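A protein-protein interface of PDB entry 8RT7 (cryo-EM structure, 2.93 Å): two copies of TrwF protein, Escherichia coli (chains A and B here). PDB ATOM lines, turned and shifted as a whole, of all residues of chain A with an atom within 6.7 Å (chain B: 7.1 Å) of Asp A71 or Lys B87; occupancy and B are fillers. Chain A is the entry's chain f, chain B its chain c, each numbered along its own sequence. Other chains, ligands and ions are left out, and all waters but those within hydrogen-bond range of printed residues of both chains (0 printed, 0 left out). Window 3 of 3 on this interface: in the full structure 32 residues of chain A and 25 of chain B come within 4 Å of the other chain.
The backbone carbonyl oxygen (O) of Gly A70 sits close to the side-chain amino group (NZ) of Lys B87 (2.3 Å). The backbone carbonyl oxygen of Gly B51 sits close to the backbone carbonyl oxygen of Gly A70, 3.1 Å away. N of Ala B53 lies within hydrogen-bond range of OD1 of Asn A96 (3.0 Å).
The side-chain carboxylate (OD2) of Asp A71 sits at hydrogen-bond distance from the backbone NH (N) of Ala A74 (2.8 Å). N of Phe B85 is in hydrogen-bond range of O of Ala B78. The backbone NH (N) of Ala B76 lies within hydrogen-bond range of the backbone carbonyl oxygen (O) of Lys B87 (2.7 Å). The side-chain carboxylate (OD2) of Asp A71 lies within hydrogen-bond range of the backbone NH (N) of Glu A73 (3.2 Å). N of Gly A70 sits at hydrogen-bond distance from O of Asn A96 (2.6 Å).
Ala A68 touches Phe B85 (CB to CD1, 3.4 Å). Ala B53 touches Phe A69 (CB to O, 3.7 Å). Phe A69 touches Lys B87. Lys B87 touches Asp A71 (NZ to CA, 3.6 Å). Gly B51 touches Thr A95 (O to CG2, 3.3 Å). Val B52 touches Asn A96 (CA to OD1, 3.3 Å).
Asp A71 touches just one residue of chain B: Lys B87. Lys B87 touches just these residues of chain A: Phe A69, Gly A70 and Asp A71. Of the printed residues of chain B, Thr A95 touches Gly B51 (3.3 Å). Of the printed residues of chain A, Gly B51 touches Gly A70 (3.1 Å) and Thr A95 (3.3 Å). Printed residues of chain A within 4 Å of Ala B53: Phe A69 (3.7 Å) and Asn A96 (3.0 Å). Ala A90 touches none of the printed residues of chain B.
Hydrophobic or aromatic side chains of chain A that line the printed part of chain B: Ala A68. Along chain A the printed residues that touch a printed residue of chain B span positions 68 to 96. Of the 21 printed residues of chain B, 5 touch a printed residue of chain A. Among the printed residues, no Asp or Glu carboxylate lies within 4 Å of a Lys or Arg side-chain nitrogen of the other chain.
Positions printed for both chains: 69, 74, 75, 76, 90 and 93. Of the 9 pairs that touch across the chains among the printed residues, none has its exchanged pair printed and touching as well.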
ATOM      1  N   ALA A  68      16.460 -17.951 -28.979  1.00  0.00           N
ATOM      2  CA  ALA A  68      15.195 -18.400 -28.410  1.00  0.00           C
ATOM      3  C   ALA A  68      14.616 -17.265 -27.592  1.00  0.00           C
ATOM      4  O   ALA A  68      15.294 -16.732 -26.710  1.00  0.00           O
ATOM      5  CB  ALA A  68      15.392 -19.641 -27.549  1.00  0.00           C
ATOM      6  N   PHE A  69      13.375 -16.896 -27.883  1.00  0.00           N
ATOM      7  CA  PHE A  69      12.703 -15.829 -27.168  1.00  0.00           C
ATOM      8  C   PHE A  69      11.925 -16.391 -25.993  1.00  0.00           C
ATOM      9  O   PHE A  69      11.590 -17.577 -25.954  1.00  0.00           O
ATOM     10  CB  PHE A  69      11.743 -15.078 -28.088  1.00  0.00           C
ATOM     11  CG  PHE A  69      12.308 -13.822 -28.664  1.00  0.00           C
ATOM     12  CD1 PHE A  69      12.776 -13.791 -29.962  1.00  0.00           C
ATOM     13  CD2 PHE A  69      12.372 -12.672 -27.906  1.00  0.00           C
ATOM     14  CE1 PHE A  69      13.292 -12.631 -30.494  1.00  0.00           C
ATOM     15  CE2 PHE A  69      12.887 -11.513 -28.427  1.00  0.00           C
ATOM     16  CZ  PHE A  69      13.347 -11.489 -29.724  1.00  0.00           C
ATOM     17  N   GLY A  70      11.633 -15.522 -25.028  1.00  0.00           N
ATOM     18  CA  GLY A  70      10.641 -15.873 -24.028  1.00  0.00           C
ATOM     19  C   GLY A  70       9.253 -15.939 -24.630  1.00  0.00           C
ATOM     20  O   GLY A  70       8.405 -16.714 -24.182  1.00  0.00           O
ATOM     21  N   ASP A  71       9.009 -15.135 -25.663  1.00  0.00           N
ATOM     22  CA  ASP A  71       7.794 -15.214 -26.473  1.00  0.00           C
ATOM     23  C   ASP A  71       8.133 -14.797 -27.898  1.00  0.00           C
ATOM     24  O   ASP A  71       8.435 -13.628 -28.153  1.00  0.00           O
ATOM     25  CB  ASP A  71       6.680 -14.354 -25.901  1.00  0.00           C
ATOM     26  CG  ASP A  71       5.335 -14.718 -26.477  1.00  0.00           C
ATOM     27  OD1 ASP A  71       4.680 -15.613 -25.927  1.00  0.00           O
ATOM     28  OD2 ASP A  71       4.934 -14.113 -27.495  1.00  0.00           O
ATOM     29  N   SER A  72       8.056 -15.753 -28.824  1.00  0.00           N
ATOM     30  CA  SER A  72       8.364 -15.457 -30.216  1.00  0.00           C
ATOM     31  C   SER A  72       7.415 -14.422 -30.799  1.00  0.00           C
ATOM     32  O   SER A  72       7.845 -13.565 -31.579  1.00  0.00           O
ATOM     33  CB  SER A  72       8.321 -16.737 -31.049  1.00  0.00           C
ATOM     34  OG  SER A  72       6.997 -17.218 -31.191  1.00  0.00           O
ATOM     35  N   GLU A  73       6.128 -14.479 -30.444  1.00  0.00           N
ATOM     36  CA  GLU A  73       5.178 -13.497 -30.949  1.00  0.00           C
ATOM     37  C   GLU A  73       5.307 -12.142 -30.274  1.00  0.00           C
ATOM     38  O   GLU A  73       4.849 -11.143 -30.839  1.00  0.00           O
ATOM     39  CB  GLU A  73       3.735 -13.976 -30.776  1.00  0.00           C
ATOM     40  CG  GLU A  73       3.497 -15.449 -30.996  1.00  0.00           C
ATOM     41  CD  GLU A  73       2.076 -15.843 -30.646  1.00  0.00           C
ATOM     42  OE1 GLU A  73       1.381 -15.039 -29.993  1.00  0.00           O
ATOM     43  OE2 GLU A  73       1.652 -16.952 -31.021  1.00  0.00           O
ATOM     44  N   ALA A  74       5.899 -12.080 -29.081  1.00  0.00           N
ATOM     45  CA  ALA A  74       5.956 -10.812 -28.364  1.00  0.00           C
ATOM     46  C   ALA A  74       6.870  -9.816 -29.064  1.00  0.00           C
ATOM     47  O   ALA A  74       6.513  -8.644 -29.222  1.00  0.00           O
ATOM     48  CB  ALA A  74       6.415 -11.038 -26.927  1.00  0.00           C
ATOM     49  N   TYR A  75       8.045 -10.260 -29.496  1.00  0.00           N
ATOM     50  CA  TYR A  75       9.035  -9.374 -30.080  1.00  0.00           C
ATOM     51  C   TYR A  75       9.302  -9.755 -31.527  1.00  0.00           C
ATOM     52  O   TYR A  75       9.027 -10.875 -31.964  1.00  0.00           O
ATOM     53  CB  TYR A  75      10.345  -9.404 -29.292  1.00  0.00           C
ATOM     54  CG  TYR A  75      10.299  -8.613 -28.015  1.00  0.00           C
ATOM     55  CD1 TYR A  75       9.999  -9.226 -26.809  1.00  0.00           C
ATOM     56  CD2 TYR A  75      10.556  -7.253 -28.012  1.00  0.00           C
ATOM     57  CE1 TYR A  75       9.955  -8.507 -25.642  1.00  0.00           C
ATOM     58  CE2 TYR A  75      10.512  -6.525 -26.853  1.00  0.00           C
ATOM     59  CZ  TYR A  75      10.212  -7.156 -25.669  1.00  0.00           C
ATOM     60  OH  TYR A  75      10.167  -6.432 -24.503  1.00  0.00           O
ATOM     61  N   ALA A  76       9.846  -8.792 -32.264  1.00  0.00           N
ATOM     62  CA  ALA A  76      10.266  -8.980 -33.642  1.00  0.00           C
ATOM     63  C   ALA A  76      11.767  -9.229 -33.681  1.00  0.00           C
ATOM     64  O   ALA A  76      12.524  -8.626 -32.918  1.00  0.00           O
ATOM     65  CB  ALA A  76       9.913  -7.758 -34.488  1.00  0.00           C
ATOM     66  N   ALA A  90       3.876  -6.624 -29.229  1.00  0.00           N
ATOM     67  CA  ALA A  90       2.689  -6.880 -28.429  1.00  0.00           C
ATOM     68  C   ALA A  90       2.853  -6.202 -27.080  1.00  0.00           C
ATOM     69  O   ALA A  90       3.955  -5.815 -26.689  1.00  0.00           O
ATOM     70  CB  ALA A  90       2.441  -8.380 -28.257  1.00  0.00           C
ATOM     71  N   ALA A  93       5.125  -7.298 -23.222  1.00  0.00           N
ATOM     72  CA  ALA A  93       6.124  -8.219 -23.757  1.00  0.00           C
ATOM     73  C   ALA A  93       7.353  -8.147 -22.859  1.00  0.00           C
ATOM     74  O   ALA A  93       8.357  -7.499 -23.165  1.00  0.00           O
ATOM     75  CB  ALA A  93       6.452  -7.883 -25.205  1.00  0.00           C
ATOM     76  N   THR A  95       9.865 -10.647 -21.494  1.00  0.00           N
ATOM     77  CA  THR A  95      10.350 -12.009 -21.669  1.00  0.00           C
ATOM     78  C   THR A  95      11.872 -11.988 -21.616  1.00  0.00           C
ATOM     79  O   THR A  95      12.488 -10.982 -21.254  1.00  0.00           O
ATOM     80  CB  THR A  95       9.825 -12.601 -22.982  1.00  0.00           C
ATOM     81  OG1 THR A  95       9.909 -11.615 -24.016  1.00  0.00           O
ATOM     82  CG2 THR A  95       8.382 -13.035 -22.829  1.00  0.00           C
ATOM     83  N   ASN A  96      12.484 -13.112 -21.976  1.00  0.00           N
ATOM     84  CA  ASN A  96      13.930 -13.247 -21.983  1.00  0.00           C
ATOM     85  C   ASN A  96      14.414 -13.615 -23.379  1.00  0.00           C
ATOM     86  O   ASN A  96      13.722 -14.299 -24.136  1.00  0.00           O
ATOM     87  CB  ASN A  96      14.401 -14.299 -20.966  1.00  0.00           C
ATOM     88  CG  ASN A  96      14.071 -15.722 -21.385  1.00  0.00           C
ATOM     89  OD1 ASN A  96      13.071 -15.973 -22.051  1.00  0.00           O
ATOM     90  ND2 ASN A  96      14.911 -16.665 -20.975  1.00  0.00           N
ATOM     91  N   THR B  48      10.787 -23.623 -13.849  1.00  0.00           N
ATOM     92  CA  THR B  48      10.414 -22.861 -15.032  1.00  0.00           C
ATOM     93  C   THR B  48       9.284 -21.904 -14.685  1.00  0.00           C
ATOM     94  O   THR B  48       8.288 -22.310 -14.081  1.00  0.00           O
ATOM     95  CB  THR B  48       9.982 -23.791 -16.165  1.00  0.00           C
ATOM     96  OG1 THR B  48       8.787 -24.481 -15.785  1.00  0.00           O
ATOM     97  CG2 THR B  48      11.063 -24.808 -16.454  1.00  0.00           C
ATOM     98  N   VAL B  49       9.446 -20.639 -15.053  1.00  0.00           N
ATOM     99  CA  VAL B  49       8.368 -19.681 -14.986  1.00  0.00           C
ATOM    100  C   VAL B  49       7.794 -19.508 -16.386  1.00  0.00           C
ATOM    101  O   VAL B  49       8.377 -19.936 -17.378  1.00  0.00           O
ATOM    102  CB  VAL B  49       8.815 -18.328 -14.391  1.00  0.00           C
ATOM    103  CG1 VAL B  49       9.300 -18.505 -12.968  1.00  0.00           C
ATOM    104  CG2 VAL B  49       9.881 -17.709 -15.233  1.00  0.00           C
ATOM    105  N   LEU B  50       6.630 -18.881 -16.468  1.00  0.00           N
ATOM    106  CA  LEU B  50       5.921 -18.767 -17.731  1.00  0.00           C
ATOM    107  C   LEU B  50       6.620 -17.771 -18.644  1.00  0.00           C
ATOM    108  O   LEU B  50       7.120 -16.739 -18.193  1.00  0.00           O
ATOM    109  CB  LEU B  50       4.479 -18.331 -17.478  1.00  0.00           C
ATOM    110  CG  LEU B  50       3.537 -18.186 -18.667  1.00  0.00           C
ATOM    111  CD1 LEU B  50       3.707 -19.348 -19.625  1.00  0.00           C
ATOM    112  CD2 LEU B  50       2.110 -18.106 -18.167  1.00  0.00           C
ATOM    113  N   GLY B  51       6.665 -18.093 -19.931  1.00  0.00           N
ATOM    114  CA  GLY B  51       7.168 -17.153 -20.912  1.00  0.00           C
ATOM    115  C   GLY B  51       8.651 -16.890 -20.864  1.00  0.00           C
ATOM    116  O   GLY B  51       9.089 -15.822 -21.299  1.00  0.00           O
ATOM    117  N   VAL B  52       9.442 -17.815 -20.328  1.00  0.00           N
ATOM    118  CA  VAL B  52      10.893 -17.721 -20.386  1.00  0.00           C
ATOM    119  C   VAL B  52      11.427 -18.997 -21.011  1.00  0.00           C
ATOM    120  O   VAL B  52      10.805 -20.062 -20.935  1.00  0.00           O
ATOM    121  CB  VAL B  52      11.540 -17.490 -19.004  1.00  0.00           C
ATOM    122  CG1 VAL B  52      10.881 -16.319 -18.297  1.00  0.00           C
ATOM    123  CG2 VAL B  52      11.497 -18.757 -18.172  1.00  0.00           C
ATOM    124  N   ALA B  53      12.584 -18.880 -21.648  1.00  0.00           N
ATOM    125  CA  ALA B  53      13.238 -20.003 -22.298  1.00  0.00           C
ATOM    126  C   ALA B  53      14.414 -20.448 -21.445  1.00  0.00           C
ATOM    127  O   ALA B  53      15.262 -19.629 -21.077  1.00  0.00           O
ATOM    128  CB  ALA B  53      13.709 -19.624 -23.701  1.00  0.00           C
ATOM    129  N   THR B  54      14.457 -21.735 -21.124  1.00  0.00           N
ATOM    130  CA  THR B  54      15.551 -22.311 -20.359  1.00  0.00           C
ATOM    131  C   THR B  54      16.514 -22.998 -21.314  1.00  0.00           C
ATOM    132  O   THR B  54      16.094 -23.797 -22.157  1.00  0.00           O
ATOM    133  CB  THR B  54      15.033 -23.302 -19.317  1.00  0.00           C
ATOM    134  OG1 THR B  54      14.265 -22.604 -18.331  1.00  0.00           O
ATOM    135  CG2 THR B  54      16.184 -24.020 -18.637  1.00  0.00           C
ATOM    136  N   PHE B  69       9.368 -36.262 -23.153  1.00  0.00           N
ATOM    137  CA  PHE B  69       8.755 -35.393 -22.168  1.00  0.00           C
ATOM    138  C   PHE B  69       7.709 -36.146 -21.358  1.00  0.00           C
ATOM    139  O   PHE B  69       7.306 -37.261 -21.690  1.00  0.00           O
ATOM    140  CB  PHE B  69       8.102 -34.202 -22.854  1.00  0.00           C
ATOM    141  CG  PHE B  69       8.952 -32.981 -22.891  1.00  0.00           C
ATOM    142  CD1 PHE B  69       9.060 -32.168 -21.787  1.00  0.00           C
ATOM    143  CD2 PHE B  69       9.618 -32.630 -24.043  1.00  0.00           C
ATOM    144  CE1 PHE B  69       9.834 -31.038 -21.825  1.00  0.00           C
ATOM    145  CE2 PHE B  69      10.391 -31.499 -24.089  1.00  0.00           C
ATOM    146  CZ  PHE B  69      10.500 -30.701 -22.979  1.00  0.00           C
ATOM    147  N   ALA B  74       2.956 -29.472 -23.016  1.00  0.00           N
ATOM    148  CA  ALA B  74       3.147 -28.477 -21.971  1.00  0.00           C
ATOM    149  C   ALA B  74       4.444 -27.704 -22.135  1.00  0.00           C
ATOM    150  O   ALA B  74       4.551 -26.578 -21.634  1.00  0.00           O
ATOM    151  CB  ALA B  74       3.124 -29.133 -20.590  1.00  0.00           C
ATOM    152  N   TYR B  75       5.431 -28.275 -22.818  1.00  0.00           N
ATOM    153  CA  TYR B  75       6.729 -27.641 -22.972  1.00  0.00           C
ATOM    154  C   TYR B  75       7.145 -27.623 -24.433  1.00  0.00           C
ATOM    155  O   TYR B  75       7.066 -28.641 -25.124  1.00  0.00           O
ATOM    156  CB  TYR B  75       7.794 -28.352 -22.141  1.00  0.00           C
ATOM    157  CG  TYR B  75       7.728 -28.012 -20.678  1.00  0.00           C
ATOM    158  CD1 TYR B  75       7.196 -28.903 -19.763  1.00  0.00           C
ATOM    159  CD2 TYR B  75       8.176 -26.786 -20.216  1.00  0.00           C
ATOM    160  CE1 TYR B  75       7.129 -28.592 -18.425  1.00  0.00           C
ATOM    161  CE2 TYR B  75       8.110 -26.463 -18.881  1.00  0.00           C
ATOM    162  CZ  TYR B  75       7.585 -27.368 -17.990  1.00  0.00           C
ATOM    163  OH  TYR B  75       7.519 -27.047 -16.658  1.00  0.00           O
ATOM    164  N   ALA B  76       7.605 -26.463 -24.889  1.00  0.00           N
ATOM    165  CA  ALA B  76       8.132 -26.310 -26.237  1.00  0.00           C
ATOM    166  C   ALA B  76       9.614 -26.656 -26.239  1.00  0.00           C
ATOM    167  O   ALA B  76      10.384 -26.106 -25.449  1.00  0.00           O
ATOM    168  CB  ALA B  76       7.922 -24.882 -26.741  1.00  0.00           C
ATOM    169  N   PHE B  77      10.010 -27.558 -27.129  1.00  0.00           N
ATOM    170  CA  PHE B  77      11.377 -28.056 -27.189  1.00  0.00           C
ATOM    171  C   PHE B  77      12.044 -27.598 -28.476  1.00  0.00           C
ATOM    172  O   PHE B  77      11.477 -27.757 -29.561  1.00  0.00           O
ATOM    173  CB  PHE B  77      11.402 -29.580 -27.115  1.00  0.00           C
ATOM    174  CG  PHE B  77      12.762 -30.151 -26.862  1.00  0.00           C
ATOM    175  CD1 PHE B  77      13.237 -30.291 -25.572  1.00  0.00           C
ATOM    176  CD2 PHE B  77      13.571 -30.534 -27.912  1.00  0.00           C
ATOM    177  CE1 PHE B  77      14.483 -30.818 -25.333  1.00  0.00           C
ATOM    178  CE2 PHE B  77      14.822 -31.061 -27.678  1.00  0.00           C
ATOM    179  CZ  PHE B  77      15.277 -31.201 -26.385  1.00  0.00           C
ATOM    180  N   ALA B  78      13.245 -27.038 -28.354  1.00  0.00           N
ATOM    181  CA  ALA B  78      14.052 -26.681 -29.511  1.00  0.00           C
ATOM    182  C   ALA B  78      15.500 -27.031 -29.220  1.00  0.00           C
ATOM    183  O   ALA B  78      16.008 -26.722 -28.140  1.00  0.00           O
ATOM    184  CB  ALA B  78      13.923 -25.194 -29.854  1.00  0.00           C
ATOM    185  N   PHE B  85      16.806 -25.851 -25.738  1.00  0.00           N
ATOM    186  CA  PHE B  85      15.933 -24.832 -25.178  1.00  0.00           C
ATOM    187  C   PHE B  85      14.574 -25.444 -24.875  1.00  0.00           C
ATOM    188  O   PHE B  85      14.078 -26.280 -25.637  1.00  0.00           O
ATOM    189  CB  PHE B  85      15.762 -23.653 -26.135  1.00  0.00           C
ATOM    190  CG  PHE B  85      17.041 -22.959 -26.479  1.00  0.00           C
ATOM    191  CD1 PHE B  85      17.424 -21.816 -25.808  1.00  0.00           C
ATOM    192  CD2 PHE B  85      17.865 -23.451 -27.473  1.00  0.00           C
ATOM    193  CE1 PHE B  85      18.600 -21.173 -26.129  1.00  0.00           C
ATOM    194  CE2 PHE B  85      19.042 -22.813 -27.793  1.00  0.00           C
ATOM    195  CZ  PHE B  85      19.409 -21.673 -27.122  1.00  0.00           C
ATOM    196  N   ILE B  86      13.978 -25.034 -23.756  1.00  0.00           N
ATOM    197  CA  ILE B  86      12.617 -25.424 -23.419  1.00  0.00           C
ATOM    198  C   ILE B  86      11.835 -24.184 -23.015  1.00  0.00           C
ATOM    199  O   ILE B  86      12.399 -23.130 -22.717  1.00  0.00           O
ATOM    200  CB  ILE B  86      12.555 -26.489 -22.305  1.00  0.00           C
ATOM    201  CG1 ILE B  86      13.023 -25.906 -20.977  1.00  0.00           C
ATOM    202  CG2 ILE B  86      13.374 -27.712 -22.676  1.00  0.00           C
ATOM    203  CD1 ILE B  86      13.240 -26.946 -19.928  1.00  0.00           C
ATOM    204  N   LYS B  87      10.508 -24.327 -23.012  1.00  0.00           N
ATOM    205  CA  LYS B  87       9.577 -23.242 -22.739  1.00  0.00           C
ATOM    206  C   LYS B  87       8.283 -23.842 -22.229  1.00  0.00           C
ATOM    207  O   LYS B  87       7.814 -24.830 -22.805  1.00  0.00           O
ATOM    208  CB  LYS B  87       9.306 -22.424 -24.003  1.00  0.00           C
ATOM    209  CG  LYS B  87       8.427 -21.213 -23.806  1.00  0.00           C
ATOM    210  CD  LYS B  87       7.598 -20.971 -25.058  1.00  0.00           C
ATOM    211  CE  LYS B  87       7.103 -19.542 -25.136  1.00  0.00           C
ATOM    212  NZ  LYS B  87       8.210 -18.613 -25.469  1.00  0.00           N
ATOM    213  N   PRO B  88       7.678 -23.289 -21.177  1.00  0.00           N
ATOM    214  CA  PRO B  88       6.374 -23.799 -20.728  1.00  0.00           C
ATOM    215  C   PRO B  88       5.260 -23.328 -21.652  1.00  0.00           C
ATOM    216  O   PRO B  88       5.095 -22.131 -21.887  1.00  0.00           O
ATOM    217  CB  PRO B  88       6.232 -23.208 -19.323  1.00  0.00           C
ATOM    218  CG  PRO B  88       7.038 -21.970 -19.368  1.00  0.00           C
ATOM    219  CD  PRO B  88       8.202 -22.252 -20.276  1.00  0.00           C
ATOM    220  N   GLN B  89       4.493 -24.284 -22.176  1.00  0.00           N
ATOM    221  CA  GLN B  89       3.436 -23.995 -23.137  1.00  0.00           C
ATOM    222  C   GLN B  89       2.036 -24.240 -22.589  1.00  0.00           C
ATOM    223  O   GLN B  89       1.064 -24.132 -23.343  1.00  0.00           O
ATOM    224  CB  GLN B  89       3.634 -24.825 -24.406  1.00  0.00           C
ATOM    225  CG  GLN B  89       4.366 -24.106 -25.517  1.00  0.00           C
ATOM    226  CD  GLN B  89       4.362 -24.899 -26.807  1.00  0.00           C
ATOM    227  OE1 GLN B  89       4.009 -26.078 -26.821  1.00  0.00           O
ATOM    228  NE2 GLN B  89       4.767 -24.260 -27.897  1.00  0.00           N
ATOM    229  N   ALA B  90       1.899 -24.567 -21.308  1.00  0.00           N
ATOM    230  CA  ALA B  90       0.585 -24.879 -20.762  1.00  0.00           C
ATOM    231  C   ALA B  90       0.571 -24.543 -19.279  1.00  0.00           C
ATOM    232  O   ALA B  90       1.616 -24.376 -18.648  1.00  0.00           O
ATOM    233  CB  ALA B  90       0.212 -26.345 -20.997  1.00  0.00           C
ATOM    234  N   ALA B  93       2.349 -26.930 -15.735  1.00  0.00           N
ATOM    235  CA  ALA B  93       3.347 -27.742 -16.424  1.00  0.00           C
ATOM    236  C   ALA B  93       4.209 -28.416 -15.368  1.00  0.00           C
ATOM    237  O   ALA B  93       5.229 -27.885 -14.929  1.00  0.00           O
ATOM    238  CB  ALA B  93       4.177 -26.889 -17.373  1.00  0.00           C
ATOM    239  N   LEU B 110      10.535 -31.098 -14.146  1.00  0.00           N
ATOM    240  CA  LEU B 110      10.030 -29.844 -14.681  1.00  0.00           C
ATOM    241  C   LEU B 110       8.795 -29.424 -13.899  1.00  0.00           C
ATOM    242  O   LEU B 110       7.762 -30.099 -13.953  1.00  0.00           O
ATOM    243  CB  LEU B 110       9.709 -29.999 -16.162  1.00  0.00           C
ATOM    244  CG  LEU B 110      10.925 -29.953 -17.081  1.00  0.00           C
ATOM    245  CD1 LEU B 110      10.640 -30.734 -18.338  1.00  0.00           C
ATOM    246  CD2 LEU B 110      11.286 -28.520 -17.402  1.00  0.00           C
